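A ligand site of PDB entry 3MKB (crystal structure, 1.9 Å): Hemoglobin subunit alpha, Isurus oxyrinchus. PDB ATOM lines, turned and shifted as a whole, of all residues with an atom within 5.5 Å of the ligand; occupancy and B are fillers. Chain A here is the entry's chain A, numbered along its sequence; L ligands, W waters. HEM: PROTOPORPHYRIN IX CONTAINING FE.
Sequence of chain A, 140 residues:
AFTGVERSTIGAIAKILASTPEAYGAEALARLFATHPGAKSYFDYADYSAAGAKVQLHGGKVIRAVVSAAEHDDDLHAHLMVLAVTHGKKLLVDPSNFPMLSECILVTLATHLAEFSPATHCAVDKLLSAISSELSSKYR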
ATOM      1  N   LEU A  32      -8.506 -14.945   6.916  1.00  0.00           N
ATOM      2  CA  LEU A  32      -7.626 -14.867   5.758  1.00  0.00           C
ATOM      3  C   LEU A  32      -6.483 -15.902   5.795  1.00  0.00           C
ATOM      4  O   LEU A  32      -6.296 -16.642   4.874  1.00  0.00           O
ATOM      5  CB  LEU A  32      -7.063 -13.469   5.597  1.00  0.00           C
ATOM      6  CG  LEU A  32      -6.238 -13.155   4.355  1.00  0.00           C
ATOM      7  CD1 LEU A  32      -6.960 -13.368   3.080  1.00  0.00           C
ATOM      8  CD2 LEU A  32      -5.612 -11.763   4.414  1.00  0.00           C
ATOM      9  N   ALA A  39      -1.415 -15.613   2.074  1.00  0.00           N
ATOM     10  CA  ALA A  39      -1.402 -14.248   2.656  1.00  0.00           C
ATOM     11  C   ALA A  39      -0.457 -14.111   3.847  1.00  0.00           C
ATOM     12  O   ALA A  39      -0.078 -13.008   4.213  1.00  0.00           O
ATOM     13  CB  ALA A  39      -2.815 -13.830   3.031  1.00  0.00           C
ATOM     14  N   TYR A  42       3.274 -12.037   3.646  1.00  0.00           N
ATOM     15  CA  TYR A  42       3.531 -10.624   3.950  1.00  0.00           C
ATOM     16  C   TYR A  42       3.920 -10.295   5.372  1.00  0.00           C
ATOM     17  O   TYR A  42       4.363  -9.174   5.634  1.00  0.00           O
ATOM     18  CB  TYR A  42       2.264  -9.777   3.605  1.00  0.00           C
ATOM     19  CG  TYR A  42       2.011  -9.806   2.127  1.00  0.00           C
ATOM     20  CD1 TYR A  42       2.781  -9.009   1.256  1.00  0.00           C
ATOM     21  CD2 TYR A  42       1.046 -10.656   1.586  1.00  0.00           C
ATOM     22  CE1 TYR A  42       2.602  -9.051  -0.087  1.00  0.00           C
ATOM     23  CE2 TYR A  42       0.836 -10.735   0.228  1.00  0.00           C
ATOM     24  CZ  TYR A  42       1.641  -9.930  -0.625  1.00  0.00           C
ATOM     25  OH  TYR A  42       1.475  -9.961  -1.969  1.00  0.00           O
ATOM     26  N   PHE A  43       3.742 -11.234   6.305  1.00  0.00           N
ATOM     27  CA  PHE A  43       3.784 -10.917   7.747  1.00  0.00           C
ATOM     28  C   PHE A  43       4.757 -11.815   8.501  1.00  0.00           C
ATOM     29  O   PHE A  43       4.676 -13.029   8.430  1.00  0.00           O
ATOM     30  CB  PHE A  43       2.372 -11.138   8.321  1.00  0.00           C
ATOM     31  CG  PHE A  43       1.311 -10.365   7.579  1.00  0.00           C
ATOM     32  CD1 PHE A  43       0.552 -10.977   6.610  1.00  0.00           C
ATOM     33  CD2 PHE A  43       1.107  -9.002   7.840  1.00  0.00           C
ATOM     34  CE1 PHE A  43      -0.425 -10.278   5.903  1.00  0.00           C
ATOM     35  CE2 PHE A  43       0.145  -8.297   7.160  1.00  0.00           C
ATOM     36  CZ  PHE A  43      -0.636  -8.956   6.169  1.00  0.00           C
ATOM     37  N   ASP A  44       5.706 -11.225   9.195  1.00  0.00           N
ATOM     38  CA  ASP A  44       6.665 -12.020   9.979  1.00  0.00           C
ATOM     39  C   ASP A  44       6.093 -12.153  11.376  1.00  0.00           C
ATOM     40  O   ASP A  44       6.529 -11.457  12.295  1.00  0.00           O
ATOM     41  CB  ASP A  44       7.997 -11.264   9.998  1.00  0.00           C
ATOM     42  CG  ASP A  44       9.101 -11.959  10.822  1.00  0.00           C
ATOM     43  OD1 ASP A  44       8.924 -13.116  11.290  1.00  0.00           O
ATOM     44  OD2 ASP A  44      10.145 -11.280  11.010  1.00  0.00           O
ATOM     45  N   TYR A  45       5.108 -13.046  11.546  1.00  0.00           N
ATOM     46  CA  TYR A  45       4.413 -13.214  12.816  1.00  0.00           C
ATOM     47  C   TYR A  45       4.791 -14.572  13.418  1.00  0.00           C
ATOM     48  O   TYR A  45       5.132 -15.498  12.699  1.00  0.00           O
ATOM     49  CB  TYR A  45       2.865 -13.215  12.662  1.00  0.00           C
ATOM     50  CG  TYR A  45       2.231 -11.913  12.205  1.00  0.00           C
ATOM     51  CD1 TYR A  45       0.884 -11.858  11.816  1.00  0.00           C
ATOM     52  CD2 TYR A  45       2.982 -10.717  12.155  1.00  0.00           C
ATOM     53  CE1 TYR A  45       0.283 -10.618  11.386  1.00  0.00           C
ATOM     54  CE2 TYR A  45       2.408  -9.516  11.707  1.00  0.00           C
ATOM     55  CZ  TYR A  45       1.063  -9.468  11.348  1.00  0.00           C
ATOM     56  OH  TYR A  45       0.491  -8.272  10.930  1.00  0.00           O
ATOM     57  N   LYS A  54       0.329  -8.796  16.915  1.00  0.00           N
ATOM     58  CA  LYS A  54       0.540  -8.079  15.680  1.00  0.00           C
ATOM     59  C   LYS A  54      -0.643  -8.218  14.718  1.00  0.00           C
ATOM     60  O   LYS A  54      -0.893  -7.347  13.879  1.00  0.00           O
ATOM     61  CB  LYS A  54       1.828  -8.571  15.026  1.00  0.00           C
ATOM     62  CG  LYS A  54       3.134  -7.907  15.507  1.00  0.00           C
ATOM     63  CD  LYS A  54       4.348  -8.748  15.019  1.00  0.00           C
ATOM     64  CE  LYS A  54       5.670  -8.181  15.525  1.00  0.00           C
ATOM     65  NZ  LYS A  54       6.795  -9.108  15.115  1.00  0.00           N
ATOM     66  N   HIS A  58      -2.723  -4.876  13.192  1.00  0.00           N
ATOM     67  CA  HIS A  58      -3.102  -4.700  11.808  1.00  0.00           C
ATOM     68  C   HIS A  58      -4.627  -4.796  11.686  1.00  0.00           C
ATOM     69  O   HIS A  58      -5.228  -4.027  10.971  1.00  0.00           O
ATOM     70  CB  HIS A  58      -2.362  -5.729  10.881  1.00  0.00           C
ATOM     71  CG  HIS A  58      -2.570  -5.485   9.412  1.00  0.00           C
ATOM     72  ND1 HIS A  58      -2.834  -6.497   8.518  1.00  0.00           N
ATOM     73  CD2 HIS A  58      -2.628  -4.332   8.704  1.00  0.00           C
ATOM     74  CE1 HIS A  58      -3.028  -5.975   7.313  1.00  0.00           C
ATOM     75  NE2 HIS A  58      -2.889  -4.669   7.399  1.00  0.00           N
ATOM     76  N   LYS A  61      -6.333  -1.470  12.572  1.00  0.00           N
ATOM     77  CA  LYS A  61      -6.014  -0.526  11.484  1.00  0.00           C
ATOM     78  C   LYS A  61      -6.859  -0.804  10.257  1.00  0.00           C
ATOM     79  O   LYS A  61      -7.414   0.129   9.670  1.00  0.00           O
ATOM     80  CB  LYS A  61      -4.537  -0.604  11.137  1.00  0.00           C
ATOM     81  CG  LYS A  61      -3.652  -0.093  12.299  1.00  0.00           C
ATOM     82  CD  LYS A  61      -2.140  -0.318  12.047  1.00  0.00           C
ATOM     83  CE  LYS A  61      -1.330   0.265  13.224  1.00  0.00           C
ATOM     84  NZ  LYS A  61       0.061  -0.174  13.045  1.00  0.00           N
ATOM     85  N   VAL A  62      -6.957  -2.083   9.831  1.00  0.00           N
ATOM     86  CA  VAL A  62      -7.900  -2.420   8.757  1.00  0.00           C
ATOM     87  C   VAL A  62      -9.341  -1.908   9.015  1.00  0.00           C
ATOM     88  O   VAL A  62      -9.908  -1.168   8.181  1.00  0.00           O
ATOM     89  CB  VAL A  62      -7.898  -3.974   8.454  1.00  0.00           C
ATOM     90  CG1 VAL A  62      -9.000  -4.329   7.452  1.00  0.00           C
ATOM     91  CG2 VAL A  62      -6.547  -4.385   7.874  1.00  0.00           C
ATOM     92  N   ALA A  65      -9.932   1.817   9.251  1.00  0.00           N
ATOM     93  CA  ALA A  65      -9.936   2.352   7.896  1.00  0.00           C
ATOM     94  C   ALA A  65     -11.230   2.064   7.113  1.00  0.00           C
ATOM     95  O   ALA A  65     -11.730   2.901   6.330  1.00  0.00           O
ATOM     96  CB  ALA A  65      -8.684   1.861   7.115  1.00  0.00           C
ATOM     97  N   VAL A  66     -11.772   0.855   7.286  1.00  0.00           N
ATOM     98  CA  VAL A  66     -13.042   0.571   6.686  1.00  0.00           C
ATOM     99  C   VAL A  66     -14.110   1.504   7.243  1.00  0.00           C
ATOM    100  O   VAL A  66     -14.930   2.006   6.469  1.00  0.00           O
ATOM    101  CB  VAL A  66     -13.490  -0.932   6.828  1.00  0.00           C
ATOM    102  CG1 VAL A  66     -14.929  -1.108   6.335  1.00  0.00           C
ATOM    103  CG2 VAL A  66     -12.566  -1.778   5.994  1.00  0.00           C
ATOM    104  N   LEU A  83      -3.755   5.289   1.384  1.00  0.00           N
ATOM    105  CA  LEU A  83      -3.647   3.891   1.658  1.00  0.00           C
ATOM    106  C   LEU A  83      -3.285   3.068   0.392  1.00  0.00           C
ATOM    107  O   LEU A  83      -2.555   2.071   0.459  1.00  0.00           O
ATOM    108  CB  LEU A  83      -4.960   3.427   2.286  1.00  0.00           C
ATOM    109  CG  LEU A  83      -4.815   2.533   3.516  1.00  0.00           C
ATOM    110  CD1 LEU A  83      -3.399   2.579   4.147  1.00  0.00           C
ATOM    111  CD2 LEU A  83      -5.907   2.928   4.482  1.00  0.00           C
ATOM    112  N   THR A  86       0.491   3.426   0.098  1.00  0.00           N
ATOM    113  CA  THR A  86       1.203   2.567   1.020  1.00  0.00           C
ATOM    114  C   THR A  86       1.142   1.100   0.594  1.00  0.00           C
ATOM    115  O   THR A  86       2.203   0.415   0.513  1.00  0.00           O
ATOM    116  CB  THR A  86       0.690   2.765   2.467  1.00  0.00           C
ATOM    117  OG1 THR A  86       0.941   4.144   2.847  1.00  0.00           O
ATOM    118  CG2 THR A  86       1.457   1.874   3.397  1.00  0.00           C
ATOM    119  N   HIS A  87      -0.068   0.614   0.274  1.00  0.00           N
ATOM    120  CA  HIS A  87      -0.199  -0.807  -0.104  1.00  0.00           C
ATOM    121  C   HIS A  87       0.376  -1.135  -1.445  1.00  0.00           C
ATOM    122  O   HIS A  87       0.998  -2.209  -1.628  1.00  0.00           O
ATOM    123  CB  HIS A  87      -1.627  -1.346   0.038  1.00  0.00           C
ATOM    124  CG  HIS A  87      -1.960  -1.673   1.458  1.00  0.00           C
ATOM    125  ND1 HIS A  87      -2.342  -0.702   2.358  1.00  0.00           N
ATOM    126  CD2 HIS A  87      -1.853  -2.818   2.157  1.00  0.00           C
ATOM    127  CE1 HIS A  87      -2.524  -1.257   3.529  1.00  0.00           C
ATOM    128  NE2 HIS A  87      -2.237  -2.535   3.454  1.00  0.00           N
ATOM    129  N   LEU A  91       4.371  -1.326   0.516  1.00  0.00           N
ATOM    130  CA  LEU A  91       4.228  -2.741   0.993  1.00  0.00           C
ATOM    131  C   LEU A  91       4.199  -3.737  -0.161  1.00  0.00           C
ATOM    132  O   LEU A  91       4.616  -4.890   0.036  1.00  0.00           O
ATOM    133  CB  LEU A  91       2.960  -2.917   1.848  1.00  0.00           C
ATOM    134  CG  LEU A  91       2.840  -1.999   3.066  1.00  0.00           C
ATOM    135  CD1 LEU A  91       1.369  -1.876   3.529  1.00  0.00           C
ATOM    136  CD2 LEU A  91       3.782  -2.524   4.181  1.00  0.00           C
ATOM    137  N   VAL A  93       1.652  -5.165  -1.825  1.00  0.00           N
ATOM    138  CA  VAL A  93       0.809  -6.351  -1.574  1.00  0.00           C
ATOM    139  C   VAL A  93       0.154  -6.732  -2.888  1.00  0.00           C
ATOM    140  O   VAL A  93      -0.396  -5.874  -3.608  1.00  0.00           O
ATOM    141  CB  VAL A  93      -0.291  -6.007  -0.509  1.00  0.00           C
ATOM    142  CG1 VAL A  93      -1.413  -7.019  -0.561  1.00  0.00           C
ATOM    143  CG2 VAL A  93       0.322  -5.733   0.912  1.00  0.00           C
ATOM    144  N   ASN A  97      -5.153 -10.064  -3.093  1.00  0.00           N
ATOM    145  CA  ASN A  97      -5.391 -10.355  -1.667  1.00  0.00           C
ATOM    146  C   ASN A  97      -6.559  -9.524  -1.151  1.00  0.00           C
ATOM    147  O   ASN A  97      -7.248  -9.945  -0.221  1.00  0.00           O
ATOM    148  CB  ASN A  97      -4.164 -10.027  -0.807  1.00  0.00           C
ATOM    149  CG  ASN A  97      -2.969 -10.948  -1.085  1.00  0.00           C
ATOM    150  OD1 ASN A  97      -2.030 -10.614  -1.871  1.00  0.00           O
ATOM    151  ND2 ASN A  97      -3.016 -12.147  -0.460  1.00  0.00           N
ATOM    152  N   PHE A  98      -6.815  -8.349  -1.741  1.00  0.00           N
ATOM    153  CA  PHE A  98      -7.902  -7.481  -1.190  1.00  0.00           C
ATOM    154  C   PHE A  98      -9.271  -8.185  -1.228  1.00  0.00           C
ATOM    155  O   PHE A  98      -9.897  -8.293  -0.246  1.00  0.00           O
ATOM    156  CB  PHE A  98      -7.901  -6.108  -1.920  1.00  0.00           C
ATOM    157  CG  PHE A  98      -6.622  -5.338  -1.622  1.00  0.00           C
ATOM    158  CD1 PHE A  98      -6.314  -5.021  -0.289  1.00  0.00           C
ATOM    159  CD2 PHE A  98      -5.699  -5.034  -2.653  1.00  0.00           C
ATOM    160  CE1 PHE A  98      -5.072  -4.312   0.067  1.00  0.00           C
ATOM    161  CE2 PHE A  98      -4.454  -4.400  -2.338  1.00  0.00           C
ATOM    162  CZ  PHE A  98      -4.122  -4.046  -0.981  1.00  0.00           C
ATOM    163  N   LEU A 101      -9.550 -10.706   1.582  1.00  0.00           N
ATOM    164  CA  LEU A 101      -9.775 -10.141   2.897  1.00  0.00           C
ATOM    165  C   LEU A 101     -11.228  -9.684   3.047  1.00  0.00           C
ATOM    166  O   LEU A 101     -11.814  -9.835   4.134  1.00  0.00           O
ATOM    167  CB  LEU A 101      -8.789  -8.997   3.223  1.00  0.00           C
ATOM    168  CG  LEU A 101      -8.886  -8.349   4.630  1.00  0.00           C
ATOM    169  CD1 LEU A 101      -8.979  -9.339   5.801  1.00  0.00           C
ATOM    170  CD2 LEU A 101      -7.719  -7.340   4.859  1.00  0.00           C
ATOM    171  N   ILE A 105     -13.882 -10.458   6.019  1.00  0.00           N
ATOM    172  CA  ILE A 105     -14.583  -9.486   6.844  1.00  0.00           C
ATOM    173  C   ILE A 105     -16.070  -9.785   6.845  1.00  0.00           C
ATOM    174  O   ILE A 105     -16.728  -9.708   7.899  1.00  0.00           O
ATOM    175  CB  ILE A 105     -14.347  -7.988   6.333  1.00  0.00           C
ATOM    176  CG1 ILE A 105     -12.910  -7.540   6.628  1.00  0.00           C
ATOM    177  CG2 ILE A 105     -15.294  -7.020   7.110  1.00  0.00           C
ATOM    178  CD1 ILE A 105     -12.483  -6.223   5.962  1.00  0.00           C
ATOM    179  N   ILE A 131     -13.550  -0.291  -1.780  1.00  0.00           N
ATOM    180  CA  ILE A 131     -12.313  -0.161  -1.054  1.00  0.00           C
ATOM    181  C   ILE A 131     -11.214  -0.949  -1.808  1.00  0.00           C
ATOM    182  O   ILE A 131     -10.209  -0.352  -2.185  1.00  0.00           O
ATOM    183  CB  ILE A 131     -12.438  -0.557   0.446  1.00  0.00           C
ATOM    184  CG1 ILE A 131     -13.393   0.406   1.188  1.00  0.00           C
ATOM    185  CG2 ILE A 131     -11.068  -0.524   1.115  1.00  0.00           C
ATOM    186  CD1 ILE A 131     -13.790  -0.078   2.571  1.00  0.00           C
ATOM    187  N   LEU A 135      -7.678   0.588  -3.206  1.00  0.00           N
ATOM    188  CA  LEU A 135      -6.427   0.030  -2.717  1.00  0.00           C
ATOM    189  C   LEU A 135      -5.570  -0.652  -3.811  1.00  0.00           C
ATOM    190  O   LEU A 135      -4.333  -0.684  -3.685  1.00  0.00           O
ATOM    191  CB  LEU A 135      -6.702  -0.950  -1.562  1.00  0.00           C
ATOM    192  CG  LEU A 135      -6.625  -0.482  -0.096  1.00  0.00           C
ATOM    193  CD1 LEU A 135      -6.868   0.984   0.133  1.00  0.00           C
ATOM    194  CD2 LEU A 135      -7.580  -1.291   0.754  1.00  0.00           C
HETATM  195  CHA HEM L   1      -0.306  -1.865   7.255  1.00  0.00           C
HETATM  196  CHB HEM L   1      -4.891  -0.826   6.216  1.00  0.00           C
HETATM  197  CHC HEM L   1      -5.370  -4.963   3.649  1.00  0.00           C
HETATM  198  CHD HEM L   1      -0.680  -5.823   4.328  1.00  0.00           C
HETATM  199  C1A HEM L   1      -1.497  -1.177   7.191  1.00  0.00           C
HETATM  200  C2A HEM L   1      -1.806   0.097   7.787  1.00  0.00           C
HETATM  201  C3A HEM L   1      -3.084   0.428   7.484  1.00  0.00           C
HETATM  202  C4A HEM L   1      -3.618  -0.685   6.718  1.00  0.00           C
HETATM  203  CMA HEM L   1      -3.893   1.719   7.868  1.00  0.00           C
HETATM  204  CAA HEM L   1      -0.714   0.924   8.483  1.00  0.00           C
HETATM  205  CBA HEM L   1      -0.249   1.752   7.241  1.00  0.00           C
HETATM  206  CGA HEM L   1       0.568   2.946   7.616  1.00  0.00           C
HETATM  207  O1A HEM L   1       1.188   2.890   8.735  1.00  0.00           O
HETATM  208  O2A HEM L   1       0.618   3.932   6.825  1.00  0.00           O
HETATM  209  C1B HEM L   1      -5.394  -1.835   5.415  1.00  0.00           C
HETATM  210  C2B HEM L   1      -6.713  -1.851   4.820  1.00  0.00           C
HETATM  211  C3B HEM L   1      -6.850  -3.002   4.145  1.00  0.00           C
HETATM  212  C4B HEM L   1      -5.627  -3.741   4.251  1.00  0.00           C
HETATM  213  CMB HEM L   1      -7.812  -0.769   4.947  1.00  0.00           C
HETATM  214  CAB HEM L   1      -8.074  -3.479   3.311  1.00  0.00           C
HETATM  215  CBB HEM L   1      -9.340  -3.074   3.455  1.00  0.00           C
HETATM  216  C1C HEM L   1      -4.148  -5.609   3.594  1.00  0.00           C
HETATM  217  C2C HEM L   1      -3.876  -6.894   2.950  1.00  0.00           C
HETATM  218  C3C HEM L   1      -2.562  -7.169   3.152  1.00  0.00           C
HETATM  219  C4C HEM L   1      -1.984  -6.060   3.917  1.00  0.00           C
HETATM  220  CMC HEM L   1      -4.988  -7.725   2.248  1.00  0.00           C
HETATM  221  CAC HEM L   1      -1.840  -8.449   2.635  1.00  0.00           C
HETATM  222  CBC HEM L   1      -2.515  -9.629   2.538  1.00  0.00           C
HETATM  223  C1D HEM L   1      -0.214  -4.868   5.230  1.00  0.00           C
HETATM  224  C2D HEM L   1       1.086  -4.955   5.845  1.00  0.00           C
HETATM  225  C3D HEM L   1       1.232  -3.812   6.798  1.00  0.00           C
HETATM  226  C4D HEM L   1       0.015  -3.051   6.605  1.00  0.00           C
HETATM  227  CMD HEM L   1       2.138  -6.084   5.647  1.00  0.00           C
HETATM  228  CAD HEM L   1       2.509  -3.565   7.687  1.00  0.00           C
HETATM  229  CBD HEM L   1       2.393  -4.021   9.179  1.00  0.00           C
HETATM  230  CGD HEM L   1       2.493  -5.540   9.482  1.00  0.00           C
HETATM  231  O1D HEM L   1       3.431  -6.262   8.989  1.00  0.00           O
HETATM  232  O2D HEM L   1       1.626  -6.071  10.232  1.00  0.00           O
HETATM  233  NA  HEM L   1      -2.623  -1.613   6.569  1.00  0.00           N
HETATM  234  NB  HEM L   1      -4.728  -3.026   5.038  1.00  0.00           N
HETATM  235  NC  HEM L   1      -2.977  -5.164   4.134  1.00  0.00           N
HETATM  236  ND  HEM L   1      -0.847  -3.712   5.702  1.00  0.00           N
HETATM  237 FE   HEM L   1      -2.824  -3.365   5.371  1.00  0.00          FE
HETATM  238  O   HOH W   1      -9.465  -5.893   1.657  1.00  0.00           O
HETATM  239  O   HOH W   2       0.960  -5.370  12.977  1.00  0.00           O
HETATM  240  O   HOH W   3      -1.070   4.780   4.605  1.00  0.00           O
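NE2 of His 87 binds FE of the ligand (2.2 Å).
OH of Tyr 45 is in hydrogen-bond range of O2D of the ligand, at 2.6 Å.
A ring nitrogen (NE2) of His 58 binds an iron atom (FE) of the ligand (2.4 Å).
The side-chain hydroxyl (OH) of Tyr 45 is in hydrogen-bond range of the backbone carbonyl oxygen (O) of Lys 54 (3.4 Å).
O of Thr 86 sits at hydrogen-bond distance from N of Leu 91 (2.8 Å).
ND1 of His 87 sits at hydrogen-bond distance from O of Leu 83 (3.4 Å).
The backbone carbonyl oxygen of His 87 is in hydrogen-bond range of the backbone NH of Val 93 (3.0 Å).
Merely in contact with the ligand: Tyr 42 (3.8 Å), Phe 43 (3.3 Å), Val 62 (3.6 Å), Ala 65 (3.5 Å), Leu 83 (3.9 Å), Thr 86 (3.997 Å), Leu 91 (3.6 Å), Val 93 (3.5 Å), Asn 97 (3.8 Å), Phe 98 (3.7 Å), Leu 101 (3.6 Å), Ile 131 (3.9 Å) and Leu 135 (3.4 Å).
Hydrophobic or aromatic side chains within 4 Å of the ligand: Tyr 42, Phe 43, Tyr 45, His 58, Val 62, Ala 65, Leu 83, His 87, Leu 91, Val 93, Phe 98, Leu 101, Ile 131 and Leu 135.
16 residues have an atom within 4 Å of the ligand: Tyr 42, Phe 43, Tyr 45, His 58, Val 62, Ala 65, Leu 83, Thr 86, His 87, Leu 91, Val 93, Asn 97, Phe 98, Leu 101, Ile 131 and Leu 135.
The nearest printed residue that does not touch the ligand is Lys 61 (4.03 Å).
Water W2 lies within hydrogen-bond range of the backbone carbonyl oxygen (O) of Lys 54 and an oxygen (O2D) of the ligand.
Water W3 bridges the side-chain hydroxyl (OG1) of Thr 86 (2.7 Å) and an oxygen (O2A) of the ligand (2.9 Å).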
